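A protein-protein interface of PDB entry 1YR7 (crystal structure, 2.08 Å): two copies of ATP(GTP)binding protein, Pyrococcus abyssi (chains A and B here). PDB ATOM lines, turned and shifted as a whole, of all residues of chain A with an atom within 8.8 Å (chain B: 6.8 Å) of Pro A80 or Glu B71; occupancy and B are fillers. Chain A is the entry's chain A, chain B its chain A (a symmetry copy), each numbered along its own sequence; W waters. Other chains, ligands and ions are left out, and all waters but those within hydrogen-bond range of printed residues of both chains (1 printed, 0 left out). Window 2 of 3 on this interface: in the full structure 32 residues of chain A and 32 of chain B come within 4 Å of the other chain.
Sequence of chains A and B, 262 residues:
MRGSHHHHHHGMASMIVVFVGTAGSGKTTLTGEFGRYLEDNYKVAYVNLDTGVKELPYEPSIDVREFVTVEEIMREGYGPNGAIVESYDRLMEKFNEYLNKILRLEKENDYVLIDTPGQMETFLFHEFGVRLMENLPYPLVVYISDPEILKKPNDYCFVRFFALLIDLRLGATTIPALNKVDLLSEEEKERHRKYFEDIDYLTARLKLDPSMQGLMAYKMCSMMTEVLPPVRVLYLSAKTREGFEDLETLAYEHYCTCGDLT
Water W1 lies within hydrogen-bond range of the side-chain hydroxyl of Thr A122 (2.5 Å) and the side-chain amide oxygen of Gln B119 (3.1 Å).
Of the 20 printed residues of chain A, 7 touch a printed residue of chain B. Printed residues of chain A that touch a printed residue of chain B: Gly A52, Val A70, Glu A71, Pro A80, Asn A81, Ile A84 and Gln A119. Of the 17 printed residues of chain B, 7 touch a printed residue of chain A. Printed residues of chain B that touch a printed residue of chain A: Gly B52, Val B70, Glu B71, Pro B80, Asn B81, Ile B84 and Gln B119.
OD1 of Asn A81 lies within hydrogen-bond range of NE2 of Gln B119 (2.9 Å). NE2 of Gln A119 sits at hydrogen-bond distance from OD1 of Asn B81 (2.9 Å).
Pro A80 touches just these residues of chain B: Gly B52 (3.8 Å), Val B70 (3.4 Å) and Glu B71 (3.4 Å). Glu B71 touches one residue of chain A. Of chain A, only Pro A80 comes within 4 Å of Gly B52. Of chain A, only Pro A80 comes within 4 Å of Val B70. Of the printed residues of chain A, Asn B81 touches Ile A84 (3.2 Å) and Gln A119 (2.9 Å). Of the printed residues of chain B, Val A70 touches Pro B80 (3.4 Å). Printed residues of chain B within 4 Å of Glu A71: Pro B80 (3.4 Å). Of the printed residues of chain B, Gln A119 touches Asn B81, Ile B84 and Gln B119. Of the printed residues of chain A, Pro B80 touches Gly A52 (3.8 Å), Val A70 (3.4 Å) and Glu A71 (3.4 Å). The nearest printed residue of chain B that does not touch Pro A80 is Pro B80 (4.5 Å). The nearest residue of chain A that does not touch Glu B71 is Gly A79 (4.5 Å).
Gly A52 touches Pro B80, and with the chains exchanged Pro A80 touches Gly B52. Glu A71 touches Pro B80, and with the chains exchanged Pro A80 touches Glu B71. Asn A81 touches Ile B84, and with the chains exchanged Ile A84 touches Asn B81. Ile A84 touches Gln B119, and with the chains exchanged Gln A119 touches Ile B84. Positions printed for both chains: 51, 52, 69, 70, 71, 73, 74, 80, 81, 83, 84 and 119.
Among the printed residues, pairs that only touch across the chains: Ile A84 with Asn B81, Asn A81 with Ile B84, Pro A80 with Glu B71, Glu A71 with Pro B80, Val A70 with Pro B80, Pro A80 with Val B70, Gln A119 with Gln B119, Pro A80 with Gly B52, Gly A52 with Pro B80, Ile A84 with Gln B119 and Gln A119 with Ile B84.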
ATOM      1  N   THR A  51     -10.104  -5.179   9.721  1.00  0.00           N
ATOM      2  CA  THR A  51     -11.165  -4.219   9.944  1.00  0.00           C
ATOM      3  C   THR A  51     -12.316  -4.780  10.760  1.00  0.00           C
ATOM      4  O   THR A  51     -12.986  -4.038  11.480  1.00  0.00           O
ATOM      5  CB  THR A  51     -11.724  -3.724   8.623  1.00  0.00           C
ATOM      6  OG1 THR A  51     -11.972  -4.851   7.773  1.00  0.00           O
ATOM      7  CG2 THR A  51     -10.733  -2.768   7.956  1.00  0.00           C
ATOM      8  N   GLY A  52     -12.546  -6.080  10.647  1.00  0.00           N
ATOM      9  CA  GLY A  52     -13.691  -6.725  11.304  1.00  0.00           C
ATOM     10  C   GLY A  52     -13.360  -7.508  12.561  1.00  0.00           C
ATOM     11  O   GLY A  52     -13.978  -8.528  12.830  1.00  0.00           O
ATOM     12  N   THR A  69     -14.773  -0.253   9.867  1.00  0.00           N
ATOM     13  CA  THR A  69     -14.940  -1.597  10.396  1.00  0.00           C
ATOM     14  C   THR A  69     -16.004  -2.311   9.587  1.00  0.00           C
ATOM     15  O   THR A  69     -16.877  -1.678   9.001  1.00  0.00           O
ATOM     16  CB  THR A  69     -15.405  -1.575  11.847  1.00  0.00           C
ATOM     17  OG1 THR A  69     -16.757  -1.128  11.876  1.00  0.00           O
ATOM     18  CG2 THR A  69     -14.556  -0.638  12.683  1.00  0.00           C
ATOM     19  N   VAL A  70     -15.924  -3.638   9.557  1.00  0.00           N
ATOM     20  CA  VAL A  70     -16.916  -4.430   8.853  1.00  0.00           C
ATOM     21  C   VAL A  70     -18.322  -4.090   9.306  1.00  0.00           C
ATOM     22  O   VAL A  70     -19.131  -3.626   8.521  1.00  0.00           O
ATOM     23  CB  VAL A  70     -16.697  -5.937   9.052  1.00  0.00           C
ATOM     24  CG1 VAL A  70     -17.986  -6.703   8.767  1.00  0.00           C
ATOM     25  CG2 VAL A  70     -15.566  -6.430   8.159  1.00  0.00           C
ATOM     26  N   GLU A  71     -18.608  -4.325  10.578  1.00  0.00           N
ATOM     27  CA  GLU A  71     -19.982  -4.270  11.067  1.00  0.00           C
ATOM     28  C   GLU A  71     -20.638  -2.902  10.844  1.00  0.00           C
ATOM     29  O   GLU A  71     -21.827  -2.822  10.506  1.00  0.00           O
ATOM     30  CB  GLU A  71     -20.048  -4.711  12.530  1.00  0.00           C
ATOM     31  CG  GLU A  71     -18.720  -4.603  13.275  1.00  0.00           C
ATOM     32  CD  GLU A  71     -17.862  -5.866  13.170  1.00  0.00           C
ATOM     33  OE1 GLU A  71     -18.247  -6.899  13.768  1.00  0.00           O
ATOM     34  OE2 GLU A  71     -16.795  -5.807  12.516  1.00  0.00           O
ATOM     35  N   ILE A  73     -19.986  -0.883   8.345  1.00  0.00           N
ATOM     36  CA  ILE A  73     -20.361  -0.890   6.935  1.00  0.00           C
ATOM     37  C   ILE A  73     -21.583  -1.767   6.690  1.00  0.00           C
ATOM     38  O   ILE A  73     -22.332  -1.543   5.740  1.00  0.00           O
ATOM     39  CB  ILE A  73     -19.210  -1.406   6.056  1.00  0.00           C
ATOM     40  CG1 ILE A  73     -18.068  -0.405   6.015  1.00  0.00           C
ATOM     41  CG2 ILE A  73     -19.667  -1.691   4.626  1.00  0.00           C
ATOM     42  CD1 ILE A  73     -16.882  -0.973   5.304  1.00  0.00           C
ATOM     43  N   MET A  74     -21.771  -2.775   7.538  1.00  0.00           N
ATOM     44  CA  MET A  74     -22.916  -3.676   7.411  1.00  0.00           C
ATOM     45  C   MET A  74     -24.238  -3.010   7.787  1.00  0.00           C
ATOM     46  O   MET A  74     -25.301  -3.441   7.345  1.00  0.00           O
ATOM     47  CB  MET A  74     -22.713  -4.932   8.249  1.00  0.00           C
ATOM     48  CG  MET A  74     -21.811  -5.938   7.586  1.00  0.00           C
ATOM     49  SD  MET A  74     -21.698  -7.468   8.502  1.00  0.00           S
ATOM     50  CE  MET A  74     -23.144  -8.339   7.879  1.00  0.00           C
ATOM     51  N   GLY A  77     -26.491  -1.971   4.850  1.00  0.00           N
ATOM     52  CA  GLY A  77     -27.177  -2.968   4.047  1.00  0.00           C
ATOM     53  C   GLY A  77     -26.263  -3.978   3.374  1.00  0.00           C
ATOM     54  O   GLY A  77     -26.715  -4.774   2.545  1.00  0.00           O
ATOM     55  N   TYR A  78     -24.980  -3.954   3.729  1.00  0.00           N
ATOM     56  CA  TYR A  78     -24.015  -4.895   3.163  1.00  0.00           C
ATOM     57  C   TYR A  78     -24.085  -6.259   3.833  1.00  0.00           C
ATOM     58  O   TYR A  78     -24.222  -6.356   5.059  1.00  0.00           O
ATOM     59  CB  TYR A  78     -22.594  -4.355   3.281  1.00  0.00           C
ATOM     60  CG  TYR A  78     -22.264  -3.225   2.338  1.00  0.00           C
ATOM     61  CD1 TYR A  78     -21.769  -3.476   1.065  1.00  0.00           C
ATOM     62  CD2 TYR A  78     -22.432  -1.903   2.730  1.00  0.00           C
ATOM     63  CE1 TYR A  78     -21.466  -2.433   0.200  1.00  0.00           C
ATOM     64  CE2 TYR A  78     -22.131  -0.862   1.887  1.00  0.00           C
ATOM     65  CZ  TYR A  78     -21.644  -1.123   0.626  1.00  0.00           C
ATOM     66  OH  TYR A  78     -21.342  -0.070  -0.210  1.00  0.00           O
ATOM     67  N   GLY A  79     -23.997  -7.305   3.015  1.00  0.00           N
ATOM     68  CA  GLY A  79     -23.797  -8.674   3.500  1.00  0.00           C
ATOM     69  C   GLY A  79     -22.390  -8.789   4.049  1.00  0.00           C
ATOM     70  O   GLY A  79     -21.536  -7.976   3.716  1.00  0.00           O
ATOM     71  N   PRO A  80     -22.137  -9.794   4.900  1.00  0.00           N
ATOM     72  CA  PRO A  80     -20.851  -9.856   5.575  1.00  0.00           C
ATOM     73  C   PRO A  80     -19.698  -9.838   4.577  1.00  0.00           C
ATOM     74  O   PRO A  80     -18.754  -9.062   4.746  1.00  0.00           O
ATOM     75  CB  PRO A  80     -20.904 -11.196   6.336  1.00  0.00           C
ATOM     76  CG  PRO A  80     -22.025 -11.951   5.740  1.00  0.00           C
ATOM     77  CD  PRO A  80     -23.004 -10.924   5.264  1.00  0.00           C
ATOM     78  N   ASN A  81     -19.790 -10.668   3.536  1.00  0.00           N
ATOM     79  CA  ASN A  81     -18.714 -10.788   2.559  1.00  0.00           C
ATOM     80  C   ASN A  81     -18.628  -9.547   1.673  1.00  0.00           C
ATOM     81  O   ASN A  81     -17.645  -9.341   0.958  1.00  0.00           O
ATOM     82  CB  ASN A  81     -18.881 -12.059   1.725  1.00  0.00           C
ATOM     83  CG  ASN A  81     -18.729 -13.316   2.553  1.00  0.00           C
ATOM     84  OD1 ASN A  81     -17.912 -13.366   3.468  1.00  0.00           O
ATOM     85  ND2 ASN A  81     -19.518 -14.337   2.243  1.00  0.00           N
ATOM     86  N   GLY A  82     -19.664  -8.715   1.742  1.00  0.00           N
ATOM     87  CA  GLY A  82     -19.693  -7.464   0.999  1.00  0.00           C
ATOM     88  C   GLY A  82     -19.072  -6.331   1.784  1.00  0.00           C
ATOM     89  O   GLY A  82     -18.374  -5.490   1.213  1.00  0.00           O
ATOM     90  N   ALA A  83     -19.339  -6.301   3.090  1.00  0.00           N
ATOM     91  CA  ALA A  83     -18.770  -5.288   3.974  1.00  0.00           C
ATOM     92  C   ALA A  83     -17.268  -5.487   4.238  1.00  0.00           C
ATOM     93  O   ALA A  83     -16.548  -4.519   4.499  1.00  0.00           O
ATOM     94  CB  ALA A  83     -19.527  -5.233   5.287  1.00  0.00           C
ATOM     95  N   ILE A  84     -16.816  -6.739   4.214  1.00  0.00           N
ATOM     96  CA  ILE A  84     -15.395  -7.046   4.322  1.00  0.00           C
ATOM     97  C   ILE A  84     -14.693  -6.409   3.134  1.00  0.00           C
ATOM     98  O   ILE A  84     -13.852  -5.522   3.300  1.00  0.00           O
ATOM     99  CB  ILE A  84     -15.127  -8.566   4.322  1.00  0.00           C
ATOM    100  CG1 ILE A  84     -15.673  -9.211   5.602  1.00  0.00           C
ATOM    101  CG2 ILE A  84     -13.633  -8.838   4.181  1.00  0.00           C
ATOM    102  CD1 ILE A  84     -15.665 -10.733   5.591  1.00  0.00           C
ATOM    103  N   VAL A  85     -15.068  -6.856   1.938  1.00  0.00           N
ATOM    104  CA  VAL A  85     -14.485  -6.371   0.700  1.00  0.00           C
ATOM    105  C   VAL A  85     -14.589  -4.856   0.627  1.00  0.00           C
ATOM    106  O   VAL A  85     -13.608  -4.170   0.335  1.00  0.00           O
ATOM    107  CB  VAL A  85     -15.128  -7.039  -0.554  1.00  0.00           C
ATOM    108  CG1 VAL A  85     -14.531  -6.469  -1.843  1.00  0.00           C
ATOM    109  CG2 VAL A  85     -14.921  -8.566  -0.505  1.00  0.00           C
ATOM    110  N   GLU A  86     -15.768  -4.334   0.933  1.00  0.00           N
ATOM    111  CA  GLU A  86     -15.964  -2.881   0.949  1.00  0.00           C
ATOM    112  C   GLU A  86     -15.066  -2.153   1.951  1.00  0.00           C
ATOM    113  O   GLU A  86     -14.706  -1.000   1.718  1.00  0.00           O
ATOM    114  CB  GLU A  86     -17.451  -2.565   1.184  1.00  0.00           C
ATOM    115  CG  GLU A  86     -17.916  -1.214   0.676  1.00  0.00           C
ATOM    116  CD  GLU A  86     -17.969  -1.104  -0.849  1.00  0.00           C
ATOM    117  OE1 GLU A  86     -17.614  -2.071  -1.566  1.00  0.00           O
ATOM    118  OE2 GLU A  86     -18.383  -0.026  -1.327  1.00  0.00           O
ATOM    119  N   SER A  87     -14.703  -2.805   3.056  1.00  0.00           N
ATOM    120  CA  SER A  87     -13.861  -2.168   4.080  1.00  0.00           C
ATOM    121  C   SER A  87     -12.446  -1.917   3.563  1.00  0.00           C
ATOM    122  O   SER A  87     -11.786  -0.948   3.954  1.00  0.00           O
ATOM    123  CB  SER A  87     -13.814  -3.003   5.377  1.00  0.00           C
ATOM    124  OG  SER A  87     -13.379  -4.344   5.142  1.00  0.00           O
ATOM    125  N   GLN A 119      -9.813 -13.187   6.930  1.00  0.00           N
ATOM    126  CA  GLN A 119      -9.747 -14.048   5.744  1.00  0.00           C
ATOM    127  C   GLN A 119      -8.488 -13.730   4.960  1.00  0.00           C
ATOM    128  O   GLN A 119      -8.265 -12.601   4.587  1.00  0.00           O
ATOM    129  CB  GLN A 119     -10.964 -13.849   4.809  1.00  0.00           C
ATOM    130  CG  GLN A 119     -12.354 -13.753   5.500  1.00  0.00           C
ATOM    131  CD  GLN A 119     -12.967 -15.105   5.815  1.00  0.00           C
ATOM    132  OE1 GLN A 119     -12.783 -16.078   5.082  1.00  0.00           O
ATOM    133  NE2 GLN A 119     -13.705 -15.172   6.915  1.00  0.00           N
ATOM    134  N   THR A 122      -8.817 -11.775   1.633  1.00  0.00           N
ATOM    135  CA  THR A 122      -8.934 -10.337   1.680  1.00  0.00           C
ATOM    136  C   THR A 122      -7.551  -9.724   1.502  1.00  0.00           C
ATOM    137  O   THR A 122      -7.410  -8.747   0.780  1.00  0.00           O
ATOM    138  CB  THR A 122      -9.547  -9.869   2.976  1.00  0.00           C
ATOM    139  OG1 THR A 122     -10.884 -10.369   3.057  1.00  0.00           O
ATOM    140  CG2 THR A 122      -9.574  -8.356   3.027  1.00  0.00           C
ATOM    141  N   THR B  51     -23.939 -19.511   2.940  1.00  0.00           N
ATOM    142  CA  THR B  51     -24.804 -19.253   4.074  1.00  0.00           C
ATOM    143  C   THR B  51     -25.100 -17.778   4.277  1.00  0.00           C
ATOM    144  O   THR B  51     -26.166 -17.423   4.780  1.00  0.00           O
ATOM    145  CB  THR B  51     -24.183 -19.788   5.351  1.00  0.00           C
ATOM    146  OG1 THR B  51     -22.813 -19.370   5.411  1.00  0.00           O
ATOM    147  CG2 THR B  51     -24.270 -21.316   5.382  1.00  0.00           C
ATOM    148  N   GLY B  52     -24.161 -16.926   3.892  1.00  0.00           N
ATOM    149  CA  GLY B  52     -24.282 -15.481   4.126  1.00  0.00           C
ATOM    150  C   GLY B  52     -24.676 -14.658   2.914  1.00  0.00           C
ATOM    151  O   GLY B  52     -24.229 -13.530   2.765  1.00  0.00           O
ATOM    152  N   VAL B  53     -25.521 -15.203   2.047  1.00  0.00           N
ATOM    153  CA  VAL B  53     -25.906 -14.494   0.833  1.00  0.00           C
ATOM    154  C   VAL B  53     -27.331 -13.962   0.936  1.00  0.00           C
ATOM    155  O   VAL B  53     -28.198 -14.592   1.532  1.00  0.00           O
ATOM    156  CB  VAL B  53     -25.743 -15.392  -0.420  1.00  0.00           C
ATOM    157  CG1 VAL B  53     -26.634 -16.631  -0.331  1.00  0.00           C
ATOM    158  CG2 VAL B  53     -26.023 -14.609  -1.690  1.00  0.00           C
ATOM    159  N   LYS B  54     -27.582 -12.804   0.335  1.00  0.00           N
ATOM    160  CA  LYS B  54     -28.872 -12.135   0.488  1.00  0.00           C
ATOM    161  C   LYS B  54     -29.900 -12.607  -0.532  1.00  0.00           C
ATOM    162  O   LYS B  54     -30.949 -13.135  -0.170  1.00  0.00           O
ATOM    163  CB  LYS B  54     -28.697 -10.614   0.410  1.00  0.00           C
ATOM    164  CG  LYS B  54     -29.455  -9.869   1.500  1.00  0.00           C
ATOM    165  CD  LYS B  54     -28.955 -10.273   2.899  1.00  0.00           C
ATOM    166  CE  LYS B  54     -30.111 -10.475   3.887  1.00  0.00           C
ATOM    167  NZ  LYS B  54     -30.970  -9.253   4.044  1.00  0.00           N
ATOM    168  N   THR B  69     -27.589 -19.179   8.655  1.00  0.00           N
ATOM    169  CA  THR B  69     -27.096 -18.041   7.896  1.00  0.00           C
ATOM    170  C   THR B  69     -26.076 -17.299   8.737  1.00  0.00           C
ATOM    171  O   THR B  69     -26.111 -17.358   9.962  1.00  0.00           O
ATOM    172  CB  THR B  69     -28.213 -17.063   7.560  1.00  0.00           C
ATOM    173  OG1 THR B  69     -28.608 -16.406   8.762  1.00  0.00           O
ATOM    174  CG2 THR B  69     -29.413 -17.777   6.972  1.00  0.00           C
ATOM    175  N   VAL B  70     -25.165 -16.599   8.068  1.00  0.00           N
ATOM    176  CA  VAL B  70     -24.167 -15.809   8.769  1.00  0.00           C
ATOM    177  C   VAL B  70     -24.808 -14.855   9.758  1.00  0.00           C
ATOM    178  O   VAL B  70     -24.579 -14.954  10.951  1.00  0.00           O
ATOM    179  CB  VAL B  70     -23.299 -14.990   7.804  1.00  0.00           C
ATOM    180  CG1 VAL B  70     -22.647 -13.822   8.537  1.00  0.00           C
ATOM    181  CG2 VAL B  70     -22.244 -15.878   7.157  1.00  0.00           C
ATOM    182  N   GLU B  71     -25.613 -13.932   9.253  1.00  0.00           N
ATOM    183  CA  GLU B  71     -26.088 -12.818  10.068  1.00  0.00           C
ATOM    184  C   GLU B  71     -26.871 -13.276  11.305  1.00  0.00           C
ATOM    185  O   GLU B  71     -26.738 -12.688  12.387  1.00  0.00           O
ATOM    186  CB  GLU B  71     -26.886 -11.831   9.213  1.00  0.00           C
ATOM    187  CG  GLU B  71     -27.438 -12.429   7.922  1.00  0.00           C
ATOM    188  CD  GLU B  71     -26.472 -12.320   6.741  1.00  0.00           C
ATOM    189  OE1 GLU B  71     -26.247 -11.185   6.257  1.00  0.00           O
ATOM    190  OE2 GLU B  71     -25.966 -13.373   6.287  1.00  0.00           O
ATOM    191  N   GLU B  72     -27.659 -14.340  11.137  1.00  0.00           N
ATOM    192  CA  GLU B  72     -28.393 -14.973  12.239  1.00  0.00           C
ATOM    193  C   GLU B  72     -27.441 -15.446  13.352  1.00  0.00           C
ATOM    194  O   GLU B  72     -27.703 -15.233  14.537  1.00  0.00           O
ATOM    195  CB  GLU B  72     -29.268 -16.106  11.682  1.00  0.00           C
ATOM    196  CG  GLU B  72     -29.368 -17.376  12.518  1.00  0.00           C
ATOM    197  CD  GLU B  72     -29.930 -18.565  11.714  1.00  0.00           C
ATOM    198  OE1 GLU B  72     -30.618 -18.351  10.683  1.00  0.00           O
ATOM    199  OE2 GLU B  72     -29.692 -19.724  12.116  1.00  0.00           O
ATOM    200  N   ILE B  73     -26.325 -16.053  12.959  1.00  0.00           N
ATOM    201  CA  ILE B  73     -25.292 -16.462  13.906  1.00  0.00           C
ATOM    202  C   ILE B  73     -24.593 -15.254  14.519  1.00  0.00           C
ATOM    203  O   ILE B  73     -24.077 -15.330  15.634  1.00  0.00           O
ATOM    204  CB  ILE B  73     -24.232 -17.343  13.227  1.00  0.00           C
ATOM    205  CG1 ILE B  73     -24.807 -18.703  12.867  1.00  0.00           C
ATOM    206  CG2 ILE B  73     -23.004 -17.546  14.113  1.00  0.00           C
ATOM    207  CD1 ILE B  73     -23.833 -19.499  12.059  1.00  0.00           C
ATOM    208  N   MET B  74     -24.561 -14.148  13.781  1.00  0.00           N
ATOM    209  CA  MET B  74     -23.929 -12.922  14.269  1.00  0.00           C
ATOM    210  C   MET B  74     -24.725 -12.249  15.386  1.00  0.00           C
ATOM    211  O   MET B  74     -24.168 -11.499  16.184  1.00  0.00           O
ATOM    212  CB  MET B  74     -23.703 -11.937  13.130  1.00  0.00           C
ATOM    213  CG  MET B  74     -22.490 -12.269  12.302  1.00  0.00           C
ATOM    214  SD  MET B  74     -22.144 -11.028  11.064  1.00  0.00           S
ATOM    215  CE  MET B  74     -21.179  -9.853  12.025  1.00  0.00           C
ATOM    216  N   ARG B  75     -26.027 -12.511  15.418  1.00  0.00           N
ATOM    217  CA  ARG B  75     -26.879 -12.081  16.510  1.00  0.00           C
ATOM    218  C   ARG B  75     -26.664 -12.985  17.728  1.00  0.00           C
ATOM    219  O   ARG B  75     -27.557 -13.146  18.557  1.00  0.00           O
ATOM    220  CB  ARG B  75     -28.355 -12.122  16.082  1.00  0.00           C
ATOM    221  CG  ARG B  75     -28.696 -11.240  14.883  1.00  0.00           C
ATOM    222  CD  ARG B  75     -30.189 -11.299  14.536  1.00  0.00           C
ATOM    223  NE  ARG B  75     -30.437 -11.077  13.104  1.00  0.00           N
ATOM    224  CZ  ARG B  75     -31.622 -10.755  12.587  1.00  0.00           C
ATOM    225  NH1 ARG B  75     -32.676 -10.604  13.384  1.00  0.00           N
ATOM    226  NH2 ARG B  75     -31.755 -10.575  11.277  1.00  0.00           N
ATOM    227  N   GLU B  76     -25.489 -13.602  17.821  1.00  0.00           N
ATOM    228  CA  GLU B  76     -25.136 -14.355  19.015  1.00  0.00           C
ATOM    229  C   GLU B  76     -23.834 -13.806  19.565  1.00  0.00           C
ATOM    230  O   GLU B  76     -23.277 -14.338  20.525  1.00  0.00           O
ATOM    231  CB  GLU B  76     -25.010 -15.846  18.719  1.00  0.00           C
ATOM    232  CG  GLU B  76     -26.296 -16.504  18.242  1.00  0.00           C
ATOM    233  CD  GLU B  76     -26.088 -17.954  17.857  1.00  0.00           C
ATOM    234  OE1 GLU B  76     -25.029 -18.507  18.221  1.00  0.00           O
ATOM    235  OE2 GLU B  76     -26.978 -18.541  17.198  1.00  0.00           O
ATOM    236  N   PRO B  80     -17.941 -11.082  12.013  1.00  0.00           N
ATOM    237  CA  PRO B  80     -18.330 -11.586  10.706  1.00  0.00           C
ATOM    238  C   PRO B  80     -17.537 -12.834  10.333  1.00  0.00           C
ATOM    239  O   PRO B  80     -18.128 -13.834   9.915  1.00  0.00           O
ATOM    240  CB  PRO B  80     -18.004 -10.419   9.754  1.00  0.00           C
ATOM    241  CG  PRO B  80     -17.120  -9.514  10.516  1.00  0.00           C
ATOM    242  CD  PRO B  80     -17.505  -9.680  11.952  1.00  0.00           C
ATOM    243  N   ASN B  81     -16.215 -12.781  10.508  1.00  0.00           N
ATOM    244  CA  ASN B  81     -15.349 -13.889  10.117  1.00  0.00           C
ATOM    245  C   ASN B  81     -15.514 -15.081  11.058  1.00  0.00           C
ATOM    246  O   ASN B  81     -15.066 -16.191  10.766  1.00  0.00           O
ATOM    247  CB  ASN B  81     -13.890 -13.434  10.042  1.00  0.00           C
ATOM    248  CG  ASN B  81     -13.661 -12.419   8.944  1.00  0.00           C
ATOM    249  OD1 ASN B  81     -14.263 -12.505   7.877  1.00  0.00           O
ATOM    250  ND2 ASN B  81     -12.792 -11.448   9.198  1.00  0.00           N
ATOM    251  N   ALA B  83     -18.770 -15.819  12.436  1.00  0.00           N
ATOM    252  CA  ALA B  83     -20.072 -16.369  12.068  1.00  0.00           C
ATOM    253  C   ALA B  83     -20.052 -17.132  10.733  1.00  0.00           C
ATOM    254  O   ALA B  83     -20.853 -18.048  10.528  1.00  0.00           O
ATOM    255  CB  ALA B  83     -21.126 -15.279  12.032  1.00  0.00           C
ATOM    256  N   ILE B  84     -19.175 -16.720   9.820  1.00  0.00           N
ATOM    257  CA  ILE B  84     -18.973 -17.439   8.569  1.00  0.00           C
ATOM    258  C   ILE B  84     -18.475 -18.833   8.912  1.00  0.00           C
ATOM    259  O   ILE B  84     -19.145 -19.830   8.625  1.00  0.00           O
ATOM    260  CB  ILE B  84     -17.944 -16.738   7.655  1.00  0.00           C
ATOM    261  CG1 ILE B  84     -18.496 -15.400   7.148  1.00  0.00           C
ATOM    262  CG2 ILE B  84     -17.576 -17.644   6.484  1.00  0.00           C
ATOM    263  CD1 ILE B  84     -17.472 -14.530   6.432  1.00  0.00           C
ATOM    264  N   GLN B 119     -16.510 -16.383   0.293  1.00  0.00           N
ATOM    265  CA  GLN B 119     -15.049 -16.486   0.404  1.00  0.00           C
ATOM    266  C   GLN B 119     -14.610 -17.878  -0.009  1.00  0.00           C
ATOM    267  O   GLN B 119     -15.074 -18.855   0.534  1.00  0.00           O
ATOM    268  CB  GLN B 119     -14.555 -16.230   1.847  1.00  0.00           C
ATOM    269  CG  GLN B 119     -15.209 -15.033   2.596  1.00  0.00           C
ATOM    270  CD  GLN B 119     -14.575 -13.694   2.267  1.00  0.00           C
ATOM    271  OE1 GLN B 119     -13.372 -13.599   2.022  1.00  0.00           O
ATOM    272  NE2 GLN B 119     -15.389 -12.647   2.260  1.00  0.00           N
HETATM  273  O   HOH W   1     -12.263 -10.914   1.000  1.00  0.00           O
